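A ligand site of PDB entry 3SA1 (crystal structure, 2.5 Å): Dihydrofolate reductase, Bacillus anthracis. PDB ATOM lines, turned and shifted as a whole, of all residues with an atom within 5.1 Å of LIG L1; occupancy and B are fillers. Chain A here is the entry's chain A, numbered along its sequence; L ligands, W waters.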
ATOM      1  N   MET A   9      18.113  24.850 -11.284  1.00  0.00           N
ATOM      2  CA  MET A   9      19.207  23.936 -10.961  1.00  0.00           C
ATOM      3  C   MET A   9      18.648  22.533 -10.999  1.00  0.00           C
ATOM      4  O   MET A   9      17.751  22.188 -10.219  1.00  0.00           O
ATOM      5  CB  MET A   9      19.804  24.254  -9.581  1.00  0.00           C
ATOM      6  CG  MET A   9      20.798  23.217  -9.059  1.00  0.00           C
ATOM      7  SD  MET A   9      22.332  23.048 -10.011  1.00  0.00           S
ATOM      8  CE  MET A   9      23.140  24.624  -9.739  1.00  0.00           C
ATOM      9  N   VAL A  10      19.167  21.722 -11.911  1.00  0.00           N
ATOM     10  CA  VAL A  10      18.562  20.426 -12.208  1.00  0.00           C
ATOM     11  C   VAL A  10      19.565  19.423 -12.791  1.00  0.00           C
ATOM     12  O   VAL A  10      20.496  19.806 -13.504  1.00  0.00           O
ATOM     13  CB  VAL A  10      17.348  20.578 -13.152  1.00  0.00           C
ATOM     14  CG1 VAL A  10      17.787  20.992 -14.567  1.00  0.00           C
ATOM     15  CG2 VAL A  10      16.528  19.285 -13.199  1.00  0.00           C
ATOM     16  N   ALA A  11      19.382  18.153 -12.441  1.00  0.00           N
ATOM     17  CA  ALA A  11      20.077  17.055 -13.085  1.00  0.00           C
ATOM     18  C   ALA A  11      19.030  16.138 -13.719  1.00  0.00           C
ATOM     19  O   ALA A  11      18.067  15.766 -13.075  1.00  0.00           O
ATOM     20  CB  ALA A  11      20.922  16.299 -12.073  1.00  0.00           C
ATOM     21  N   ILE A  18      14.066  12.902 -13.846  1.00  0.00           N
ATOM     22  CA  ILE A  18      14.704  13.519 -12.672  1.00  0.00           C
ATOM     23  C   ILE A  18      14.397  12.778 -11.350  1.00  0.00           C
ATOM     24  O   ILE A  18      15.077  12.988 -10.350  1.00  0.00           O
ATOM     25  CB  ILE A  18      14.367  15.043 -12.527  1.00  0.00           C
ATOM     26  CG1 ILE A  18      12.876  15.256 -12.205  1.00  0.00           C
ATOM     27  CG2 ILE A  18      14.814  15.831 -13.769  1.00  0.00           C
ATOM     28  CD1 ILE A  18      12.536  16.638 -11.727  1.00  0.00           C
ATOM     29  N   GLY A  19      13.379  11.906 -11.368  1.00  0.00           N
ATOM     30  CA  GLY A  19      12.941  11.192 -10.168  1.00  0.00           C
ATOM     31  C   GLY A  19      12.258   9.838 -10.374  1.00  0.00           C
ATOM     32  O   GLY A  19      11.641   9.564 -11.407  1.00  0.00           O
ATOM     33  N   LYS A  20      12.400   8.980  -9.370  1.00  0.00           N
ATOM     34  CA  LYS A  20      11.749   7.665  -9.338  1.00  0.00           C
ATOM     35  C   LYS A  20      11.313   7.454  -7.897  1.00  0.00           C
ATOM     36  O   LYS A  20      12.121   7.621  -6.973  1.00  0.00           O
ATOM     37  CB  LYS A  20      12.754   6.578  -9.747  1.00  0.00           C
ATOM     38  CG  LYS A  20      12.191   5.158  -9.844  1.00  0.00           C
ATOM     39  CD  LYS A  20      13.286   4.130  -9.470  1.00  0.00           C
ATOM     40  CE  LYS A  20      13.137   2.759 -10.166  1.00  0.00           C
ATOM     41  NZ  LYS A  20      11.823   2.046  -9.902  1.00  0.00           N
ATOM     42  N   ASP A  21      10.041   7.118  -7.721  1.00  0.00           N
ATOM     43  CA  ASP A  21       9.455   6.849  -6.398  1.00  0.00           C
ATOM     44  C   ASP A  21       9.823   7.906  -5.356  1.00  0.00           C
ATOM     45  O   ASP A  21      10.288   7.559  -4.257  1.00  0.00           O
ATOM     46  CB  ASP A  21       9.825   5.434  -5.905  1.00  0.00           C
ATOM     47  CG  ASP A  21       9.365   4.317  -6.865  1.00  0.00           C
ATOM     48  OD1 ASP A  21       8.239   4.410  -7.421  1.00  0.00           O
ATOM     49  OD2 ASP A  21      10.121   3.343  -7.045  1.00  0.00           O
ATOM     50  N   ASN A  22       9.622   9.177  -5.703  1.00  0.00           N
ATOM     51  CA  ASN A  22       9.875  10.338  -4.804  1.00  0.00           C
ATOM     52  C   ASN A  22      11.317  10.482  -4.301  1.00  0.00           C
ATOM     53  O   ASN A  22      11.565  11.027  -3.222  1.00  0.00           O
ATOM     54  CB  ASN A  22       8.859  10.372  -3.639  1.00  0.00           C
ATOM     55  CG  ASN A  22       8.589  11.792  -3.147  1.00  0.00           C
ATOM     56  OD1 ASN A  22       8.836  12.771  -3.864  1.00  0.00           O
ATOM     57  ND2 ASN A  22       8.075  11.899  -1.927  1.00  0.00           N
ATOM     58  N   ASN A  23      12.266  10.022  -5.117  1.00  0.00           N
ATOM     59  CA  ASN A  23      13.689  10.050  -4.789  1.00  0.00           C
ATOM     60  C   ASN A  23      14.495  10.219  -6.080  1.00  0.00           C
ATOM     61  O   ASN A  23      13.930  10.238  -7.178  1.00  0.00           O
ATOM     62  CB  ASN A  23      14.082   8.741  -4.093  1.00  0.00           C
ATOM     63  CG  ASN A  23      15.180   8.919  -3.013  1.00  0.00           C
ATOM     64  OD1 ASN A  23      16.064   9.782  -3.108  1.00  0.00           O
ATOM     65  ND2 ASN A  23      15.121   8.060  -1.988  1.00  0.00           N
ATOM     66  N   LEU A  24      15.816  10.338  -5.936  1.00  0.00           N
ATOM     67  CA  LEU A  24      16.760  10.387  -7.044  1.00  0.00           C
ATOM     68  C   LEU A  24      17.086   9.004  -7.587  1.00  0.00           C
ATOM     69  O   LEU A  24      17.305   8.078  -6.811  1.00  0.00           O
ATOM     70  CB  LEU A  24      18.061  11.064  -6.594  1.00  0.00           C
ATOM     71  CG  LEU A  24      17.980  12.540  -6.209  1.00  0.00           C
ATOM     72  CD1 LEU A  24      19.276  12.916  -5.523  1.00  0.00           C
ATOM     73  CD2 LEU A  24      17.704  13.455  -7.431  1.00  0.00           C
ATOM     74  N   TRP A  26      19.765   8.029  -9.160  1.00  0.00           N
ATOM     75  CA  TRP A  26      21.206   7.782  -9.237  1.00  0.00           C
ATOM     76  C   TRP A  26      21.920   8.359  -8.006  1.00  0.00           C
ATOM     77  O   TRP A  26      21.388   9.214  -7.312  1.00  0.00           O
ATOM     78  CB  TRP A  26      21.777   8.421 -10.508  1.00  0.00           C
ATOM     79  CG  TRP A  26      21.376   9.869 -10.635  1.00  0.00           C
ATOM     80  CD1 TRP A  26      21.936  10.937  -9.974  1.00  0.00           C
ATOM     81  CD2 TRP A  26      20.320  10.401 -11.433  1.00  0.00           C
ATOM     82  NE1 TRP A  26      21.295  12.098 -10.319  1.00  0.00           N
ATOM     83  CE2 TRP A  26      20.298  11.798 -11.221  1.00  0.00           C
ATOM     84  CE3 TRP A  26      19.377   9.841 -12.314  1.00  0.00           C
ATOM     85  CZ2 TRP A  26      19.366  12.646 -11.855  1.00  0.00           C
ATOM     86  CZ3 TRP A  26      18.454  10.692 -12.951  1.00  0.00           C
ATOM     87  CH2 TRP A  26      18.454  12.068 -12.708  1.00  0.00           C
ATOM     88  N   GLY A  47       9.917  22.552  -4.129  1.00  0.00           N
ATOM     89  CA  GLY A  47       8.574  22.029  -3.988  1.00  0.00           C
ATOM     90  C   GLY A  47       8.473  21.236  -2.705  1.00  0.00           C
ATOM     91  O   GLY A  47       9.474  20.654  -2.274  1.00  0.00           O
ATOM     92  N   ARG A  48       7.289  21.230  -2.090  1.00  0.00           N
ATOM     93  CA  ARG A  48       7.081  20.547  -0.805  1.00  0.00           C
ATOM     94  C   ARG A  48       7.617  19.122  -0.840  1.00  0.00           C
ATOM     95  O   ARG A  48       8.409  18.747   0.028  1.00  0.00           O
ATOM     96  CB  ARG A  48       5.597  20.591  -0.391  1.00  0.00           C
ATOM     97  CG  ARG A  48       5.298  20.251   1.077  1.00  0.00           C
ATOM     98  CD  ARG A  48       4.922  18.776   1.269  1.00  0.00           C
ATOM     99  NE  ARG A  48       3.754  18.378   0.472  1.00  0.00           N
ATOM    100  CZ  ARG A  48       3.428  17.124   0.189  1.00  0.00           C
ATOM    101  NH1 ARG A  48       4.184  16.125   0.623  1.00  0.00           N
ATOM    102  NH2 ARG A  48       2.342  16.851  -0.529  1.00  0.00           N
ATOM    103  N   LYS A  49       7.231  18.345  -1.850  1.00  0.00           N
ATOM    104  CA  LYS A  49       7.669  16.961  -1.995  1.00  0.00           C
ATOM    105  C   LYS A  49       9.200  16.862  -2.064  1.00  0.00           C
ATOM    106  O   LYS A  49       9.805  16.139  -1.263  1.00  0.00           O
ATOM    107  CB  LYS A  49       7.011  16.280  -3.200  1.00  0.00           C
ATOM    108  CG  LYS A  49       5.571  15.853  -2.936  1.00  0.00           C
ATOM    109  CD  LYS A  49       5.176  14.712  -3.847  1.00  0.00           C
ATOM    110  CE  LYS A  49       3.672  14.712  -4.143  1.00  0.00           C
ATOM    111  NZ  LYS A  49       3.296  13.631  -5.114  1.00  0.00           N
ATOM    112  N   ASN A  50       9.813  17.605  -2.996  1.00  0.00           N
ATOM    113  CA  ASN A  50      11.257  17.708  -3.058  1.00  0.00           C
ATOM    114  C   ASN A  50      11.836  17.990  -1.678  1.00  0.00           C
ATOM    115  O   ASN A  50      12.744  17.273  -1.251  1.00  0.00           O
ATOM    116  CB  ASN A  50      11.710  18.796  -4.040  1.00  0.00           C
ATOM    117  CG  ASN A  50      13.225  18.939  -4.113  1.00  0.00           C
ATOM    118  OD1 ASN A  50      13.955  17.998  -3.823  1.00  0.00           O
ATOM    119  ND2 ASN A  50      13.703  20.111  -4.500  1.00  0.00           N
ATOM    120  N   ALA A  53      11.710  14.994   0.744  1.00  0.00           N
ATOM    121  CA  ALA A  53      12.651  13.963   0.325  1.00  0.00           C
ATOM    122  C   ALA A  53      14.078  14.345   0.734  1.00  0.00           C
ATOM    123  O   ALA A  53      14.867  13.481   1.111  1.00  0.00           O
ATOM    124  CB  ALA A  53      12.553  13.729  -1.167  1.00  0.00           C
ATOM    125  N   VAL A  66       7.638  25.526  -1.265  1.00  0.00           N
ATOM    126  CA  VAL A  66       6.413  25.894  -1.969  1.00  0.00           C
ATOM    127  C   VAL A  66       5.315  24.843  -1.772  1.00  0.00           C
ATOM    128  O   VAL A  66       5.502  23.668  -2.110  1.00  0.00           O
ATOM    129  CB  VAL A  66       6.675  26.163  -3.461  1.00  0.00           C
ATOM    130  CG1 VAL A  66       5.416  26.713  -4.134  1.00  0.00           C
ATOM    131  CG2 VAL A  66       7.848  27.122  -3.631  1.00  0.00           C
ATOM    132  N   THR A  67       4.184  25.301  -1.238  1.00  0.00           N
ATOM    133  CA  THR A  67       3.075  24.436  -0.865  1.00  0.00           C
ATOM    134  C   THR A  67       1.752  25.212  -0.926  1.00  0.00           C
ATOM    135  O   THR A  67       1.732  26.421  -0.771  1.00  0.00           O
ATOM    136  CB  THR A  67       3.295  23.853   0.553  1.00  0.00           C
ATOM    137  OG1 THR A  67       2.173  23.046   0.931  1.00  0.00           O
ATOM    138  CG2 THR A  67       3.490  24.952   1.588  1.00  0.00           C
ATOM    139  N   ARG A  68       0.640  24.512  -1.161  1.00  0.00           N
ATOM    140  CA  ARG A  68      -0.682  25.146  -1.202  1.00  0.00           C
ATOM    141  C   ARG A  68      -1.279  25.157   0.199  1.00  0.00           C
ATOM    142  O   ARG A  68      -2.322  25.771   0.426  1.00  0.00           O
ATOM    143  CB  ARG A  68      -1.616  24.415  -2.163  1.00  0.00           C
ATOM    144  CG  ARG A  68      -1.371  24.652  -3.646  1.00  0.00           C
ATOM    145  CD  ARG A  68      -2.420  23.914  -4.494  1.00  0.00           C
ATOM    146  NE  ARG A  68      -2.174  24.061  -5.927  1.00  0.00           N
ATOM    147  CZ  ARG A  68      -1.463  23.210  -6.664  1.00  0.00           C
ATOM    148  NH1 ARG A  68      -0.925  22.132  -6.106  1.00  0.00           N
ATOM    149  NH2 ARG A  68      -1.276  23.434  -7.957  1.00  0.00           N
ATOM    150  N   ASN A  69      -0.607  24.463   1.112  1.00  0.00           N
ATOM    151  CA  ASN A  69      -1.020  24.251   2.492  1.00  0.00           C
ATOM    152  C   ASN A  69      -0.650  25.478   3.348  1.00  0.00           C
ATOM    153  O   ASN A  69       0.529  25.745   3.593  1.00  0.00           O
ATOM    154  CB  ASN A  69      -0.318  22.981   3.015  1.00  0.00           C
ATOM    155  CG  ASN A  69      -0.792  22.522   4.379  1.00  0.00           C
ATOM    156  OD1 ASN A  69      -1.429  23.251   5.136  1.00  0.00           O
ATOM    157  ND2 ASN A  69      -0.470  21.282   4.713  1.00  0.00           N
ATOM    158  N   HIS A  81       3.583  30.194  -0.963  1.00  0.00           N
ATOM    159  CA  HIS A  81       2.412  29.484  -1.415  1.00  0.00           C
ATOM    160  C   HIS A  81       2.106  29.782  -2.869  1.00  0.00           C
ATOM    161  O   HIS A  81       1.124  29.278  -3.407  1.00  0.00           O
ATOM    162  CB  HIS A  81       1.211  29.800  -0.515  1.00  0.00           C
ATOM    163  CG  HIS A  81       1.472  29.523   0.935  1.00  0.00           C
ATOM    164  ND1 HIS A  81       1.953  30.485   1.804  1.00  0.00           N
ATOM    165  CD2 HIS A  81       1.326  28.391   1.674  1.00  0.00           C
ATOM    166  CE1 HIS A  81       2.088  29.954   3.010  1.00  0.00           C
ATOM    167  NE2 HIS A  81       1.705  28.694   2.958  1.00  0.00           N
ATOM    168  N   SER A  82       2.970  30.582  -3.492  1.00  0.00           N
ATOM    169  CA  SER A  82       2.804  30.954  -4.893  1.00  0.00           C
ATOM    170  C   SER A  82       4.101  31.579  -5.440  1.00  0.00           C
ATOM    171  O   SER A  82       4.988  31.950  -4.676  1.00  0.00           O
ATOM    172  CB  SER A  82       1.626  31.938  -5.057  1.00  0.00           C
ATOM    173  OG  SER A  82       1.952  33.226  -4.562  1.00  0.00           O
ATOM    174  N   PHE A  99      14.864  24.690  -7.531  1.00  0.00           N
ATOM    175  CA  PHE A  99      15.617  23.511  -7.159  1.00  0.00           C
ATOM    176  C   PHE A  99      14.788  22.233  -7.327  1.00  0.00           C
ATOM    177  O   PHE A  99      15.275  21.144  -7.055  1.00  0.00           O
ATOM    178  CB  PHE A  99      16.070  23.671  -5.704  1.00  0.00           C
ATOM    179  CG  PHE A  99      17.234  22.800  -5.301  1.00  0.00           C
ATOM    180  CD1 PHE A  99      18.477  22.924  -5.931  1.00  0.00           C
ATOM    181  CD2 PHE A  99      17.105  21.881  -4.254  1.00  0.00           C
ATOM    182  CE1 PHE A  99      19.552  22.124  -5.553  1.00  0.00           C
ATOM    183  CE2 PHE A  99      18.191  21.066  -3.870  1.00  0.00           C
ATOM    184  CZ  PHE A  99      19.412  21.192  -4.521  1.00  0.00           C
ATOM    185  N   GLY A 100      13.542  22.371  -7.786  1.00  0.00           N
ATOM    186  CA  GLY A 100      12.693  21.217  -8.100  1.00  0.00           C
ATOM    187  C   GLY A 100      11.620  20.912  -7.073  1.00  0.00           C
ATOM    188  O   GLY A 100      11.519  21.592  -6.050  1.00  0.00           O
ATOM    189  N   GLY A 101      10.797  19.895  -7.318  1.00  0.00           N
ATOM    190  CA  GLY A 101      10.916  19.023  -8.480  1.00  0.00           C
ATOM    191  C   GLY A 101      10.146  19.509  -9.690  1.00  0.00           C
ATOM    192  O   GLY A 101      10.134  20.699  -9.975  1.00  0.00           O
ATOM    193  N   ALA A 102       9.495  18.577 -10.399  1.00  0.00           N
ATOM    194  CA  ALA A 102       8.842  18.882 -11.665  1.00  0.00           C
ATOM    195  C   ALA A 102       7.734  19.936 -11.579  1.00  0.00           C
ATOM    196  O   ALA A 102       7.697  20.853 -12.402  1.00  0.00           O
ATOM    197  CB  ALA A 102       8.301  17.612 -12.298  1.00  0.00           C
ATOM    198  N   GLN A 103       6.837  19.795 -10.600  1.00  0.00           N
ATOM    199  CA  GLN A 103       5.725  20.737 -10.474  1.00  0.00           C
ATOM    200  C   GLN A 103       6.217  22.147 -10.246  1.00  0.00           C
ATOM    201  O   GLN A 103       5.683  23.092 -10.823  1.00  0.00           O
ATOM    202  CB  GLN A 103       4.757  20.344  -9.369  1.00  0.00           C
ATOM    203  CG  GLN A 103       3.998  19.050  -9.643  1.00  0.00           C
ATOM    204  CD  GLN A 103       2.984  18.746  -8.557  1.00  0.00           C
ATOM    205  OE1 GLN A 103       2.149  19.589  -8.224  1.00  0.00           O
ATOM    206  NE2 GLN A 103       3.045  17.557  -8.003  1.00  0.00           N
ATOM    207  N   ILE A 104       7.270  22.287  -9.438  1.00  0.00           N
ATOM    208  CA  ILE A 104       7.876  23.590  -9.157  1.00  0.00           C
ATOM    209  C   ILE A 104       8.670  24.136 -10.354  1.00  0.00           C
ATOM    210  O   ILE A 104       8.667  25.359 -10.579  1.00  0.00           O
ATOM    211  CB  ILE A 104       8.660  23.595  -7.805  1.00  0.00           C
ATOM    212  CG1 ILE A 104       7.803  24.249  -6.719  1.00  0.00           C
ATOM    213  CG2 ILE A 104       9.961  24.324  -7.880  1.00  0.00           C
ATOM    214  CD1 ILE A 104       6.501  23.500  -6.437  1.00  0.00           C
ATOM    215  N   TYR A 105       9.306  23.257 -11.132  1.00  0.00           N
ATOM    216  CA  TYR A 105       9.934  23.691 -12.403  1.00  0.00           C
ATOM    217  C   TYR A 105       8.871  24.217 -13.370  1.00  0.00           C
ATOM    218  O   TYR A 105       9.079  25.267 -13.958  1.00  0.00           O
ATOM    219  CB  TYR A 105      10.765  22.606 -13.097  1.00  0.00           C
ATOM    220  CG  TYR A 105      12.009  22.153 -12.384  1.00  0.00           C
ATOM    221  CD1 TYR A 105      12.988  23.057 -11.963  1.00  0.00           C
ATOM    222  CD2 TYR A 105      12.224  20.803 -12.145  1.00  0.00           C
ATOM    223  CE1 TYR A 105      14.134  22.625 -11.292  1.00  0.00           C
ATOM    224  CE2 TYR A 105      13.358  20.353 -11.497  1.00  0.00           C
ATOM    225  CZ  TYR A 105      14.303  21.267 -11.064  1.00  0.00           C
ATOM    226  OH  TYR A 105      15.422  20.792 -10.423  1.00  0.00           O
ATOM    227  N   LEU A 107       6.099  25.516 -12.514  1.00  0.00           N
ATOM    228  CA  LEU A 107       5.595  26.775 -11.943  1.00  0.00           C
ATOM    229  C   LEU A 107       6.383  27.987 -12.389  1.00  0.00           C
ATOM    230  O   LEU A 107       5.791  29.018 -12.727  1.00  0.00           O
ATOM    231  CB  LEU A 107       5.597  26.743 -10.404  1.00  0.00           C
ATOM    232  CG  LEU A 107       4.267  26.653  -9.663  1.00  0.00           C
ATOM    233  CD1 LEU A 107       4.511  27.003  -8.200  1.00  0.00           C
ATOM    234  CD2 LEU A 107       3.163  27.544 -10.272  1.00  0.00           C
ATOM    235  N   THR A 128       9.159  10.902 -12.808  1.00  0.00           N
ATOM    236  CA  THR A 128       9.142  12.354 -12.788  1.00  0.00           C
ATOM    237  C   THR A 128      10.124  12.921 -13.808  1.00  0.00           C
ATOM    238  O   THR A 128      11.235  12.412 -13.953  1.00  0.00           O
ATOM    239  CB  THR A 128       9.400  12.897 -11.365  1.00  0.00           C
ATOM    240  OG1 THR A 128       8.421  12.335 -10.476  1.00  0.00           O
ATOM    241  CG2 THR A 128       9.270  14.416 -11.319  1.00  0.00           C
HETATM  242  P1  LIG L   1       7.613  18.923  -6.136  1.00  0.00           P
HETATM  243  O1  LIG L   1       7.438  19.785  -7.334  1.00  0.00           O
HETATM  244  O2  LIG L   1       8.944  19.047  -5.524  1.00  0.00           O
HETATM  245  O3  LIG L   1       6.486  19.248  -5.068  1.00  0.00           O
HETATM  246  C1  LIG L   1       5.123  19.100  -5.408  1.00  0.00           C
HETATM  247  C2  LIG L   1       4.368  19.963  -4.418  1.00  0.00           C
HETATM  248  O4  LIG L   1       4.649  21.317  -4.691  1.00  0.00           O
HETATM  249  C3  LIG L   1       2.857  19.856  -4.412  1.00  0.00           C
HETATM  250  O5  LIG L   1       2.420  18.762  -3.660  1.00  0.00           O
HETATM  251  C4  LIG L   1       2.500  21.142  -3.706  1.00  0.00           C
HETATM  252  O6  LIG L   1       2.667  20.991  -2.323  1.00  0.00           O
HETATM  253  C5  LIG L   1       3.575  22.105  -4.232  1.00  0.00           C
HETATM  254  N1  LIG L   1       3.016  22.872  -5.364  1.00  0.00           N
HETATM  255  C6  LIG L   1       2.895  22.449  -6.656  1.00  0.00           C
HETATM  256  N2  LIG L   1       2.318  23.441  -7.379  1.00  0.00           N
HETATM  257  C7  LIG L   1       2.068  24.475  -6.539  1.00  0.00           C
HETATM  258  C8  LIG L   1       1.494  25.717  -6.744  1.00  0.00           C
HETATM  259  N3  LIG L   1       1.096  26.038  -7.965  1.00  0.00           N
HETATM  260  N4  LIG L   1       1.364  26.596  -5.687  1.00  0.00           N
HETATM  261  C9  LIG L   1       1.798  26.250  -4.434  1.00  0.00           C
HETATM  262  N5  LIG L   1       2.371  25.003  -4.238  1.00  0.00           N
HETATM  263  C10 LIG L   1       2.503  24.133  -5.277  1.00  0.00           C
HETATM  264  O7  LIG L   1       7.222  17.404  -6.493  1.00  0.00           O
HETATM  265  P2  LIG L   1       7.394  16.554  -7.849  1.00  0.00           P
HETATM  266  O8  LIG L   1       6.794  15.219  -7.595  1.00  0.00           O
HETATM  267  O9  LIG L   1       6.914  17.410  -8.973  1.00  0.00           O
HETATM  268  O10 LIG L   1       8.999  16.360  -7.923  1.00  0.00           O
HETATM  269  C11 LIG L   1       9.610  15.589  -6.900  1.00  0.00           C
HETATM  270  C12 LIG L   1      10.518  14.517  -7.476  1.00  0.00           C
HETATM  271  O11 LIG L   1      11.599  15.077  -8.230  1.00  0.00           O
HETATM  272  C13 LIG L   1      11.175  13.729  -6.359  1.00  0.00           C
HETATM  273  O12 LIG L   1      11.388  12.416  -6.843  1.00  0.00           O
HETATM  274  C14 LIG L   1      12.521  14.398  -6.212  1.00  0.00           C
HETATM  275  O13 LIG L   1      13.458  13.539  -5.607  1.00  0.00           O
HETATM  276  C15 LIG L   1      12.842  14.741  -7.650  1.00  0.00           C
HETATM  277  N6  LIG L   1      13.775  15.858  -7.835  1.00  0.00           N
HETATM  278  C16 LIG L   1      14.855  15.685  -8.646  1.00  0.00           C
HETATM  279  C17 LIG L   1      15.754  16.714  -8.869  1.00  0.00           C
HETATM  280  C18 LIG L   1      16.862  16.526  -9.860  1.00  0.00           C
HETATM  281  O14 LIG L   1      17.551  17.656 -10.349  1.00  0.00           O
HETATM  282  N7  LIG L   1      17.161  15.281 -10.257  1.00  0.00           N
HETATM  283  C19 LIG L   1      15.549  17.958  -8.268  1.00  0.00           C
HETATM  284  C20 LIG L   1      14.447  18.137  -7.446  1.00  0.00           C
HETATM  285  C21 LIG L   1      13.559  17.070  -7.237  1.00  0.00           C
HETATM  286  P3  LIG L   1       1.507  20.572  -1.289  1.00  0.00           P
HETATM  287  O15 LIG L   1       1.017  19.191  -1.568  1.00  0.00           O
HETATM  288  O16 LIG L   1       2.119  20.595   0.090  1.00  0.00           O
HETATM  289  O17 LIG L   1       0.306  21.501  -1.430  1.00  0.00           O
HETATM  290  N1  LG2 L   2      20.073  19.820  -9.307  1.00  0.00           N
HETATM  291  C1  LG2 L   2      21.132  19.083  -9.688  1.00  0.00           C
HETATM  292  N2  LG2 L   2      21.389  17.910  -9.092  1.00  0.00           N
HETATM  293  C2  LG2 L   2      20.616  17.421  -8.103  1.00  0.00           C
HETATM  294  C3  LG2 L   2      19.501  18.172  -7.698  1.00  0.00           C
HETATM  295  C4  LG2 L   2      19.240  19.404  -8.326  1.00  0.00           C
HETATM  296  C5  LG2 L   2      21.969  16.205  -6.328  1.00  0.00           C
HETATM  297  C6  LG2 L   2      16.501  13.285  -2.009  1.00  0.00           C
HETATM  298  N3  LG2 L   2      21.945  19.484 -10.647  1.00  0.00           N
HETATM  299  N4  LG2 L   2      18.200  20.156  -7.968  1.00  0.00           N
HETATM  300  C7  LG2 L   2      17.972  17.205  -5.751  1.00  0.00           C
HETATM  301  C8  LG2 L   2      18.672  17.672  -6.659  1.00  0.00           C
HETATM  302  C9  LG2 L   2      22.518  18.511   0.130  1.00  0.00           C
HETATM  303  C10 LG2 L   2      22.276  19.753  -1.809  1.00  0.00           C
HETATM  304  C11 LG2 L   2      21.515  17.625  -0.274  1.00  0.00           C
HETATM  305  C12 LG2 L   2      21.268  18.899  -2.276  1.00  0.00           C
HETATM  306  C13 LG2 L   2      19.683  15.717  -1.230  1.00  0.00           C
HETATM  307  C14 LG2 L   2      18.705  14.816  -1.617  1.00  0.00           C
HETATM  308  C15 LG2 L   2      19.026  17.180  -3.030  1.00  0.00           C
HETATM  309  C16 LG2 L   2      21.030  16.057  -7.529  1.00  0.00           C
HETATM  310  C17 LG2 L   2      17.153  16.642  -4.667  1.00  0.00           C
HETATM  311  N5  LG2 L   2      22.864  19.548  -0.623  1.00  0.00           N
HETATM  312  O1  LG2 L   2      16.920  14.161  -3.077  1.00  0.00           O
HETATM  313  C18 LG2 L   2      20.862  17.811  -1.497  1.00  0.00           C
HETATM  314  C19 LG2 L   2      19.863  16.914  -1.930  1.00  0.00           C
HETATM  315  C20 LG2 L   2      18.030  16.268  -3.444  1.00  0.00           C
HETATM  316  C21 LG2 L   2      17.869  15.086  -2.709  1.00  0.00           C
HETATM  317  O   HOH W   1      14.442  15.417  -3.718  1.00  0.00           O
HETATM  318  O   HOH W   2      -1.752  20.968  -3.525  1.00  0.00           O
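O16 of LIG L1 lies within hydrogen-bond range of OG1 of Thr 67 (2.6 Å). An oxygen (O2) of LIG L1 sits at hydrogen-bond distance from the backbone NH of Gly 101 (2.7 Å). The guanidinium group (NE) of Arg 48 is in salt-bridge range of an oxygen (O16) of LIG L1. O14 of LIG L1 lies within hydrogen-bond range of N of Ala 11 (2.8 Å). A nitrogen (N7) of LIG L1 is in hydrogen-bond range of the backbone carbonyl oxygen (O) of Ala 11, at 3.0 Å. An oxygen (O9) of LIG L1 sits at hydrogen-bond distance from the backbone NH (N) of Gln 103 (2.9 Å). N of Asn 50 sits at hydrogen-bond distance from O2 of LIG L1. N of Arg 68 lies within hydrogen-bond range of O17 of LIG L1 (3.0 Å). An oxygen (O12) of LIG L1 is in hydrogen-bond range of the backbone NH of Asn 23 (3.1 Å). O of Asn 23 is in hydrogen-bond range of O12 of LIG L1. A nitrogen (N7) of LIG L1 sits at hydrogen-bond distance from the backbone carbonyl oxygen (O) of Ile 18 (3.1 Å). N of Ala 102 lies within hydrogen-bond range of O9 of LIG L1. An oxygen (O1) of LIG L1 is in hydrogen-bond range of the backbone NH (N) of Ile 104 (3.3 Å). An oxygen (O3) of LIG L1 lies within hydrogen-bond range of the backbone NH (N) of Lys 49, at 3.4 Å. The backbone carbonyl oxygen (O) of Phe 99 sits at hydrogen-bond distance from a nitrogen (N4) of LG2 L2, 3.2 Å away. The backbone NH of Val 10 sits close to a nitrogen (N1) of LG2 L2, at 3.3 Å. N3 of LG2 L2 lies close to O of Val 10 (3.2 Å). N4 of LG2 L2 lies within hydrogen-bond range of O of Met 9 (3.1 Å). SD of Met 9 is in hydrogen-bond range of N3 of LG2 L2 (3.6 Å).
N of Asn 69 sits at hydrogen-bond distance from OG1 of Thr 67 (3.1 Å). The backbone NH of Arg 48 is in hydrogen-bond range of the backbone carbonyl oxygen of Val 66. The backbone carbonyl oxygen (O) of Phe 99 sits at hydrogen-bond distance from the side-chain amide nitrogen (ND2) of Asn 50, at 3.2 Å. O of Phe 99 is in hydrogen-bond range of OH of Tyr 105 (3.4 Å). The backbone carbonyl oxygen (O) of Asn 69 sits at hydrogen-bond distance from a ring nitrogen (NE2) of His 81 (3.2 Å). The backbone NH of Gly 47 sits at hydrogen-bond distance from the backbone carbonyl oxygen of Gly 100 (2.7 Å). The side-chain hydroxyl of Tyr 105 sits at hydrogen-bond distance from the backbone carbonyl oxygen of Met 9 (2.7 Å). The backbone NH (N) of Thr 128 is in hydrogen-bond range of the backbone carbonyl oxygen (O) of Gly 19 (3.1 Å).
CG2 of Val 10 touches O14 of LIG L1, 3.4 Å away. Gly 19 touches LIG L1 (CA to O12, 3.9 Å). C of Asn 22 touches O12 of LIG L1, 3.2 Å away. Leu 24 touches LIG L1 (CD2 to N7, 3.4 Å). CZ2 of Trp 26 touches N7 of LIG L1, at 3.8 Å. CA of Gly 47 touches O2 of LIG L1 (3.4 Å). Val 66 touches LIG L1. His 81 touches LIG L1 (O to C9, 3.3 Å). Phe 99 touches LIG L1. CA of Gly 100 touches C20 of LIG L1, 3.6 Å away. OH of Tyr 105 touches C19 of LIG L1, at 3.6 Å. CD2 of Leu 107 touches N3 of LIG L1, 3.4 Å away. CG2 of Thr 128 touches O10 of LIG L1, at 3.9 Å. Hydrophobic or aromatic side chains within 4 Å of LIG L1: Val 10, Ile 18, Leu 24, Trp 26, Val 66, Ala 102, Ile 104 and Leu 107. The nearest printed residue that does not touch LIG L1 is Asn 69 (4.01 Å).
Water W1 lies within hydrogen-bond range of OD1 of Asn 50 (2.6 Å), O13 of LIG L1 (2.8 Å) and O1 of LG2 L2 (2.9 Å). Water W2 lies within hydrogen-bond range of the guanidinium group (NH1) of Arg 68 (2.9 Å) and an oxygen (O17) of LIG L1 (3.0 Å).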
